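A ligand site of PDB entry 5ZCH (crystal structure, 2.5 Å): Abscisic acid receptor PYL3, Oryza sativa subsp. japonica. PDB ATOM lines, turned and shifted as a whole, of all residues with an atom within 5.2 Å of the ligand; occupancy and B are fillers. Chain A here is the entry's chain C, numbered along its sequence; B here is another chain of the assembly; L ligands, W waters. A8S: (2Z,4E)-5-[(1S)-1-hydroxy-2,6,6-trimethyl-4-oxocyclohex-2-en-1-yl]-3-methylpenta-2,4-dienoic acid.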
ATOM      1  N   LYS A  47      26.901  -1.427  18.975  1.00  0.00           N
ATOM      2  CA  LYS A  47      25.942  -1.516  17.882  1.00  0.00           C
ATOM      3  C   LYS A  47      24.859  -2.540  18.225  1.00  0.00           C
ATOM      4  O   LYS A  47      25.179  -3.722  18.419  1.00  0.00           O
ATOM      5  CB  LYS A  47      26.641  -1.901  16.583  1.00  0.00           C
ATOM      6  CG  LYS A  47      27.665  -0.879  16.107  1.00  0.00           C
ATOM      7  CD  LYS A  47      27.866  -0.948  14.610  1.00  0.00           C
ATOM      8  CE  LYS A  47      28.909   0.068  14.148  1.00  0.00           C
ATOM      9  NZ  LYS A  47      29.132   0.019  12.685  1.00  0.00           N
ATOM     10  N   PHE A  49      22.538  -3.917  16.413  1.00  0.00           N
ATOM     11  CA  PHE A  49      22.131  -4.826  15.350  1.00  0.00           C
ATOM     12  C   PHE A  49      23.109  -5.972  15.119  1.00  0.00           C
ATOM     13  O   PHE A  49      22.727  -6.950  14.478  1.00  0.00           O
ATOM     14  CB  PHE A  49      21.980  -4.055  14.035  1.00  0.00           C
ATOM     15  CG  PHE A  49      21.069  -2.861  14.133  1.00  0.00           C
ATOM     16  CD1 PHE A  49      19.707  -3.026  14.316  1.00  0.00           C
ATOM     17  CD2 PHE A  49      21.585  -1.578  14.039  1.00  0.00           C
ATOM     18  CE1 PHE A  49      18.873  -1.927  14.405  1.00  0.00           C
ATOM     19  CE2 PHE A  49      20.758  -0.475  14.125  1.00  0.00           C
ATOM     20  CZ  PHE A  49      19.394  -0.652  14.315  1.00  0.00           C
ATOM     21  N   VAL A  69      24.135  -9.629  11.324  1.00  0.00           N
ATOM     22  CA  VAL A  69      23.169  -8.782  12.010  1.00  0.00           C
ATOM     23  C   VAL A  69      21.953  -9.621  12.386  1.00  0.00           C
ATOM     24  O   VAL A  69      21.669 -10.665  11.789  1.00  0.00           O
ATOM     25  CB  VAL A  69      22.756  -7.560  11.165  1.00  0.00           C
ATOM     26  CG1 VAL A  69      23.944  -6.616  10.993  1.00  0.00           C
ATOM     27  CG2 VAL A  69      22.211  -7.989   9.826  1.00  0.00           C
ATOM     28  N   LEU A  73      15.820  -7.226   9.927  1.00  0.00           N
ATOM     29  CA  LEU A  73      16.429  -6.208   9.095  1.00  0.00           C
ATOM     30  C   LEU A  73      16.413  -6.626   7.632  1.00  0.00           C
ATOM     31  O   LEU A  73      16.243  -7.800   7.308  1.00  0.00           O
ATOM     32  CB  LEU A  73      17.876  -5.948   9.555  1.00  0.00           C
ATOM     33  CG  LEU A  73      18.012  -5.356  10.957  1.00  0.00           C
ATOM     34  CD1 LEU A  73      19.402  -5.592  11.510  1.00  0.00           C
ATOM     35  CD2 LEU A  73      17.661  -3.868  10.949  1.00  0.00           C
ATOM     36  N   PRO A  74      16.585  -5.678   6.699  1.00  0.00           N
ATOM     37  CA  PRO A  74      16.597  -6.043   5.276  1.00  0.00           C
ATOM     38  C   PRO A  74      17.766  -6.924   4.874  1.00  0.00           C
ATOM     39  O   PRO A  74      17.706  -7.549   3.810  1.00  0.00           O
ATOM     40  CB  PRO A  74      16.647  -4.682   4.555  1.00  0.00           C
ATOM     41  CG  PRO A  74      16.154  -3.702   5.557  1.00  0.00           C
ATOM     42  CD  PRO A  74      16.586  -4.212   6.892  1.00  0.00           C
ATOM     43  N   ALA A  75      18.818  -6.985   5.686  1.00  0.00           N
ATOM     44  CA  ALA A  75      20.005  -7.772   5.371  1.00  0.00           C
ATOM     45  C   ALA A  75      20.347  -8.672   6.550  1.00  0.00           C
ATOM     46  O   ALA A  75      19.800  -8.540   7.649  1.00  0.00           O
ATOM     47  CB  ALA A  75      21.194  -6.878   5.013  1.00  0.00           C
ATOM     48  N   ARG A  77      24.025  -9.968   6.681  1.00  0.00           N
ATOM     49  CA  ARG A  77      25.465  -9.964   6.841  1.00  0.00           C
ATOM     50  C   ARG A  77      26.063  -8.772   6.115  1.00  0.00           C
ATOM     51  O   ARG A  77      25.440  -8.200   5.215  1.00  0.00           O
ATOM     52  CB  ARG A  77      26.097 -11.274   6.343  1.00  0.00           C
ATOM     53  CG  ARG A  77      25.850 -11.546   4.864  1.00  0.00           C
ATOM     54  CD  ARG A  77      26.557 -12.814   4.423  1.00  0.00           C
ATOM     55  NE  ARG A  77      26.128 -13.236   3.093  1.00  0.00           N
ATOM     56  CZ  ARG A  77      26.669 -12.799   1.953  1.00  0.00           C
ATOM     57  NH1 ARG A  77      27.670 -11.925   1.992  1.00  0.00           N
ATOM     58  NH2 ARG A  77      26.213 -13.240   0.786  1.00  0.00           N
ATOM     59  N   SER A  78      27.284  -8.405   6.499  1.00  0.00           N
ATOM     60  CA  SER A  78      27.998  -7.310   5.864  1.00  0.00           C
ATOM     61  C   SER A  78      29.494  -7.501   6.030  1.00  0.00           C
ATOM     62  O   SER A  78      29.955  -7.974   7.070  1.00  0.00           O
ATOM     63  CB  SER A  78      27.569  -5.962   6.445  1.00  0.00           C
ATOM     64  OG  SER A  78      28.396  -4.914   5.955  1.00  0.00           O
ATOM     65  N   GLU A  80      33.064  -5.364   5.895  1.00  0.00           N
ATOM     66  CA  GLU A  80      33.473  -3.978   6.062  1.00  0.00           C
ATOM     67  C   GLU A  80      34.987  -3.887   6.237  1.00  0.00           C
ATOM     68  O   GLU A  80      35.603  -4.729   6.890  1.00  0.00           O
ATOM     69  CB  GLU A  80      32.760  -3.342   7.273  1.00  0.00           C
ATOM     70  CG  GLU A  80      31.299  -3.752   7.397  1.00  0.00           C
ATOM     71  CD  GLU A  80      30.662  -3.344   8.707  1.00  0.00           C
ATOM     72  OE1 GLU A  80      29.454  -3.039   8.709  1.00  0.00           O
ATOM     73  OE2 GLU A  80      31.376  -3.317   9.730  1.00  0.00           O
ATOM     74  N   PHE A  96      32.072  -0.318   3.317  1.00  0.00           N
ATOM     75  CA  PHE A  96      31.429  -1.612   3.137  1.00  0.00           C
ATOM     76  C   PHE A  96      31.855  -2.189   1.786  1.00  0.00           C
ATOM     77  O   PHE A  96      31.657  -1.555   0.747  1.00  0.00           O
ATOM     78  CB  PHE A  96      29.904  -1.483   3.212  1.00  0.00           C
ATOM     79  CG  PHE A  96      29.389  -1.063   4.561  1.00  0.00           C
ATOM     80  CD1 PHE A  96      30.246  -0.910   5.635  1.00  0.00           C
ATOM     81  CD2 PHE A  96      28.039  -0.832   4.754  1.00  0.00           C
ATOM     82  CE1 PHE A  96      29.771  -0.525   6.879  1.00  0.00           C
ATOM     83  CE2 PHE A  96      27.558  -0.439   5.995  1.00  0.00           C
ATOM     84  CZ  PHE A  96      28.424  -0.286   7.057  1.00  0.00           C
ATOM     85  N   HIS A 101      23.338  -6.758   1.691  1.00  0.00           N
ATOM     86  CA  HIS A 101      22.537  -5.555   1.863  1.00  0.00           C
ATOM     87  C   HIS A 101      22.444  -4.778   0.556  1.00  0.00           C
ATOM     88  O   HIS A 101      22.981  -5.189  -0.476  1.00  0.00           O
ATOM     89  CB  HIS A 101      23.120  -4.681   2.977  1.00  0.00           C
ATOM     90  CG  HIS A 101      24.592  -4.471   2.861  1.00  0.00           C
ATOM     91  ND1 HIS A 101      25.137  -3.449   2.105  1.00  0.00           N
ATOM     92  CD2 HIS A 101      25.645  -5.134   3.407  1.00  0.00           C
ATOM     93  CE1 HIS A 101      26.458  -3.499   2.191  1.00  0.00           C
ATOM     94  NE2 HIS A 101      26.782  -4.514   2.969  1.00  0.00           N
ATOM     95  N   LEU A 103      23.374  -1.426   0.400  1.00  0.00           N
ATOM     96  CA  LEU A 103      24.190  -0.238   0.598  1.00  0.00           C
ATOM     97  C   LEU A 103      25.538  -0.474  -0.092  1.00  0.00           C
ATOM     98  O   LEU A 103      26.534  -0.832   0.540  1.00  0.00           O
ATOM     99  CB  LEU A 103      24.362   0.069   2.094  1.00  0.00           C
ATOM    100  CG  LEU A 103      23.102   0.459   2.865  1.00  0.00           C
ATOM    101  CD1 LEU A 103      23.439   0.806   4.310  1.00  0.00           C
ATOM    102  CD2 LEU A 103      22.391   1.616   2.183  1.00  0.00           C
ATOM    103  N   TYR A 106      29.131   1.943   0.316  1.00  0.00           N
ATOM    104  CA  TYR A 106      28.912   2.729   1.523  1.00  0.00           C
ATOM    105  C   TYR A 106      30.249   3.081   2.171  1.00  0.00           C
ATOM    106  O   TYR A 106      31.101   2.213   2.371  1.00  0.00           O
ATOM    107  CB  TYR A 106      28.043   1.944   2.508  1.00  0.00           C
ATOM    108  CG  TYR A 106      27.788   2.644   3.834  1.00  0.00           C
ATOM    109  CD1 TYR A 106      28.697   2.530   4.881  1.00  0.00           C
ATOM    110  CD2 TYR A 106      26.633   3.391   4.046  1.00  0.00           C
ATOM    111  CE1 TYR A 106      28.467   3.156   6.099  1.00  0.00           C
ATOM    112  CE2 TYR A 106      26.397   4.019   5.252  1.00  0.00           C
ATOM    113  CZ  TYR A 106      27.320   3.894   6.282  1.00  0.00           C
ATOM    114  OH  TYR A 106      27.085   4.519   7.479  1.00  0.00           O
ATOM    115  N   GLU A 127      28.760  11.320  12.692  1.00  0.00           N
ATOM    116  CA  GLU A 127      28.949  10.245  11.723  1.00  0.00           C
ATOM    117  C   GLU A 127      28.264  10.633  10.423  1.00  0.00           C
ATOM    118  O   GLU A 127      27.047  10.842  10.405  1.00  0.00           O
ATOM    119  CB  GLU A 127      28.416   8.907  12.243  1.00  0.00           C
ATOM    120  CG  GLU A 127      28.425   7.801  11.199  1.00  0.00           C
ATOM    121  CD  GLU A 127      28.525   6.420  11.820  1.00  0.00           C
ATOM    122  OE1 GLU A 127      29.494   5.701  11.505  1.00  0.00           O
ATOM    123  OE2 GLU A 127      27.635   6.055  12.613  1.00  0.00           O
ATOM    124  N   PHE A 145      16.706   5.904   5.585  1.00  0.00           N
ATOM    125  CA  PHE A 145      16.994   4.567   6.075  1.00  0.00           C
ATOM    126  C   PHE A 145      18.324   4.531   6.831  1.00  0.00           C
ATOM    127  O   PHE A 145      18.390   4.001   7.952  1.00  0.00           O
ATOM    128  CB  PHE A 145      17.015   3.569   4.912  1.00  0.00           C
ATOM    129  CG  PHE A 145      17.434   2.184   5.304  1.00  0.00           C
ATOM    130  CD1 PHE A 145      16.737   1.490   6.278  1.00  0.00           C
ATOM    131  CD2 PHE A 145      18.525   1.573   4.704  1.00  0.00           C
ATOM    132  CE1 PHE A 145      17.122   0.216   6.649  1.00  0.00           C
ATOM    133  CE2 PHE A 145      18.905   0.302   5.063  1.00  0.00           C
ATOM    134  CZ  PHE A 145      18.202  -0.380   6.043  1.00  0.00           C
ATOM    135  N   VAL A 146      19.378   5.098   6.241  1.00  0.00           N
ATOM    136  CA  VAL A 146      20.690   5.063   6.886  1.00  0.00           C
ATOM    137  C   VAL A 146      20.688   5.913   8.153  1.00  0.00           C
ATOM    138  O   VAL A 146      21.279   5.533   9.171  1.00  0.00           O
ATOM    139  CB  VAL A 146      21.778   5.524   5.892  1.00  0.00           C
ATOM    140  CG1 VAL A 146      23.129   5.563   6.579  1.00  0.00           C
ATOM    141  CG2 VAL A 146      21.809   4.596   4.696  1.00  0.00           C
ATOM    142  N   LEU A 149      19.243   4.030  11.139  1.00  0.00           N
ATOM    143  CA  LEU A 149      20.158   3.046  11.717  1.00  0.00           C
ATOM    144  C   LEU A 149      21.280   3.730  12.492  1.00  0.00           C
ATOM    145  O   LEU A 149      21.675   3.264  13.562  1.00  0.00           O
ATOM    146  CB  LEU A 149      20.729   2.154  10.618  1.00  0.00           C
ATOM    147  CG  LEU A 149      19.720   1.285   9.866  1.00  0.00           C
ATOM    148  CD1 LEU A 149      20.408   0.558   8.721  1.00  0.00           C
ATOM    149  CD2 LEU A 149      19.049   0.301  10.803  1.00  0.00           C
ATOM    150  N   LEU A 150      21.812   4.839  11.960  1.00  0.00           N
ATOM    151  CA  LEU A 150      22.916   5.513  12.607  1.00  0.00           C
ATOM    152  C   LEU A 150      22.496   6.148  13.931  1.00  0.00           C
ATOM    153  O   LEU A 150      23.241   6.123  14.912  1.00  0.00           O
ATOM    154  CB  LEU A 150      23.528   6.561  11.672  1.00  0.00           C
ATOM    155  CG  LEU A 150      24.206   6.028  10.423  1.00  0.00           C
ATOM    156  CD1 LEU A 150      24.913   7.135   9.660  1.00  0.00           C
ATOM    157  CD2 LEU A 150      25.191   4.923  10.782  1.00  0.00           C
ATOM    158  N   ASN A 153      22.375   3.496  16.361  1.00  0.00           N
ATOM    159  CA  ASN A 153      23.735   3.143  16.771  1.00  0.00           C
ATOM    160  C   ASN A 153      24.279   4.138  17.782  1.00  0.00           C
ATOM    161  O   ASN A 153      24.823   3.751  18.825  1.00  0.00           O
ATOM    162  CB  ASN A 153      24.648   3.076  15.542  1.00  0.00           C
ATOM    163  CG  ASN A 153      24.580   1.746  14.828  1.00  0.00           C
ATOM    164  OD1 ASN A 153      23.987   0.786  15.321  1.00  0.00           O
ATOM    165  ND2 ASN A 153      25.196   1.668  13.659  1.00  0.00           N
ATOM    166  N   TRP B 202      12.228  -1.583   0.389  1.00  0.00           N
ATOM    167  CA  TRP B 202      13.641  -1.875   0.603  1.00  0.00           C
ATOM    168  C   TRP B 202      13.740  -3.358   0.962  1.00  0.00           C
ATOM    169  O   TRP B 202      13.711  -3.715   2.144  1.00  0.00           O
ATOM    170  CB  TRP B 202      14.230  -0.980   1.695  1.00  0.00           C
ATOM    171  CG  TRP B 202      15.720  -0.937   1.726  1.00  0.00           C
ATOM    172  CD1 TRP B 202      16.562  -1.936   2.134  1.00  0.00           C
ATOM    173  CD2 TRP B 202      16.561   0.169   1.364  1.00  0.00           C
ATOM    174  NE1 TRP B 202      17.871  -1.520   2.028  1.00  0.00           N
ATOM    175  CE2 TRP B 202      17.889  -0.230   1.563  1.00  0.00           C
ATOM    176  CE3 TRP B 202      16.305   1.457   0.887  1.00  0.00           C
ATOM    177  CZ2 TRP B 202      18.971   0.611   1.307  1.00  0.00           C
ATOM    178  CZ3 TRP B 202      17.373   2.301   0.630  1.00  0.00           C
ATOM    179  CH2 TRP B 202      18.687   1.872   0.843  1.00  0.00           C
HETATM  180  C1  A8S L   1      26.729   1.067  10.748  1.00  0.00           C
HETATM  181  C2  A8S L   1      25.789   1.645   9.699  1.00  0.00           C
HETATM  182  C3  A8S L   1      24.858   0.974   8.997  1.00  0.00           C
HETATM  183  C4  A8S L   1      24.633  -0.456   9.151  1.00  0.00           C
HETATM  184  C5  A8S L   1      23.936  -1.166   8.269  1.00  0.00           C
HETATM  185  C6  A8S L   1      24.031   1.716   8.014  1.00  0.00           C
HETATM  186  C7  A8S L   1      23.716  -2.636   8.443  1.00  0.00           C
HETATM  187  O7  A8S L   1      24.574  -3.258   9.358  1.00  0.00           O
HETATM  188  C8  A8S L   1      22.305  -2.850   8.950  1.00  0.00           C
HETATM  189  C9  A8S L   1      21.261  -2.912   8.120  1.00  0.00           C
HETATM  190  C10 A8S L   1      21.434  -2.954   6.665  1.00  0.00           C
HETATM  191  O10 A8S L   1      20.466  -3.027   5.919  1.00  0.00           O
HETATM  192  C11 A8S L   1      22.843  -2.885   6.106  1.00  0.00           C
HETATM  193  O11 A8S L   1      27.782   1.730  11.011  1.00  0.00           O
HETATM  194  C12 A8S L   1      23.949  -3.355   7.081  1.00  0.00           C
HETATM  195  O12 A8S L   1      26.441  -0.001  11.305  1.00  0.00           O
HETATM  196  C13 A8S L   1      22.061  -2.589  10.388  1.00  0.00           C
HETATM  197  C14 A8S L   1      23.876  -4.873   7.212  1.00  0.00           C
HETATM  198  C15 A8S L   1      25.297  -2.994   6.481  1.00  0.00           C
HETATM  199  O   HOH W   1      28.808   3.617   9.542  1.00  0.00           O
HETATM  200  O   HOH W   2      20.051  -3.418   2.920  1.00  0.00           O
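NZ of Lys 47 lies within salt-bridge range of O11 of the ligand, at 2.7 Å. ND2 of Asn 153 is in hydrogen-bond range of O12 of the ligand (3.1 Å).
The backbone NH (N) of Phe 96 sits at hydrogen-bond distance from the backbone carbonyl oxygen (O) of Tyr 106, at 2.9 Å. A ring nitrogen (NE2) of His 101 lies within hydrogen-bond range of the side-chain hydroxyl (OG) of Ser 78. A ring nitrogen (ND1) of His 101 is in hydrogen-bond range of the backbone NH (N) of Leu 103. OG of Ser 78 sits close to OE1 of Glu 80, 3.5 Å away.
Phe 49 touches the ligand. Val 69 touches the ligand (CG1 to O7, 3.8 Å). OG of Ser 78 touches C15 of the ligand (3.7 Å). CE2 of Phe 96 touches C15 of the ligand, at 3.4 Å. His 101 touches the ligand (CB to C11, 3.6 Å). Leu 103 touches the ligand (CD1 to C6, 3.9 Å). OH of Tyr 106 touches C2 of the ligand, 3.9 Å away. Phe 145 touches the ligand (CZ to O10, 3.5 Å). CD1 of Leu 149 touches C9 of the ligand (3.6 Å). Leu 150 touches the ligand (CD2 to C2, 3.5 Å). Of the 20 residues printed, 12 come within 4 Å of the ligand.
Water W1 lies within hydrogen-bond range of O11 of the ligand, OH of Tyr 106 and OE1 of Glu 127. Water W2 bridges NE1 of Trp 202 of chain B (3.0 Å) and O10 of the ligand (3.1 Å).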
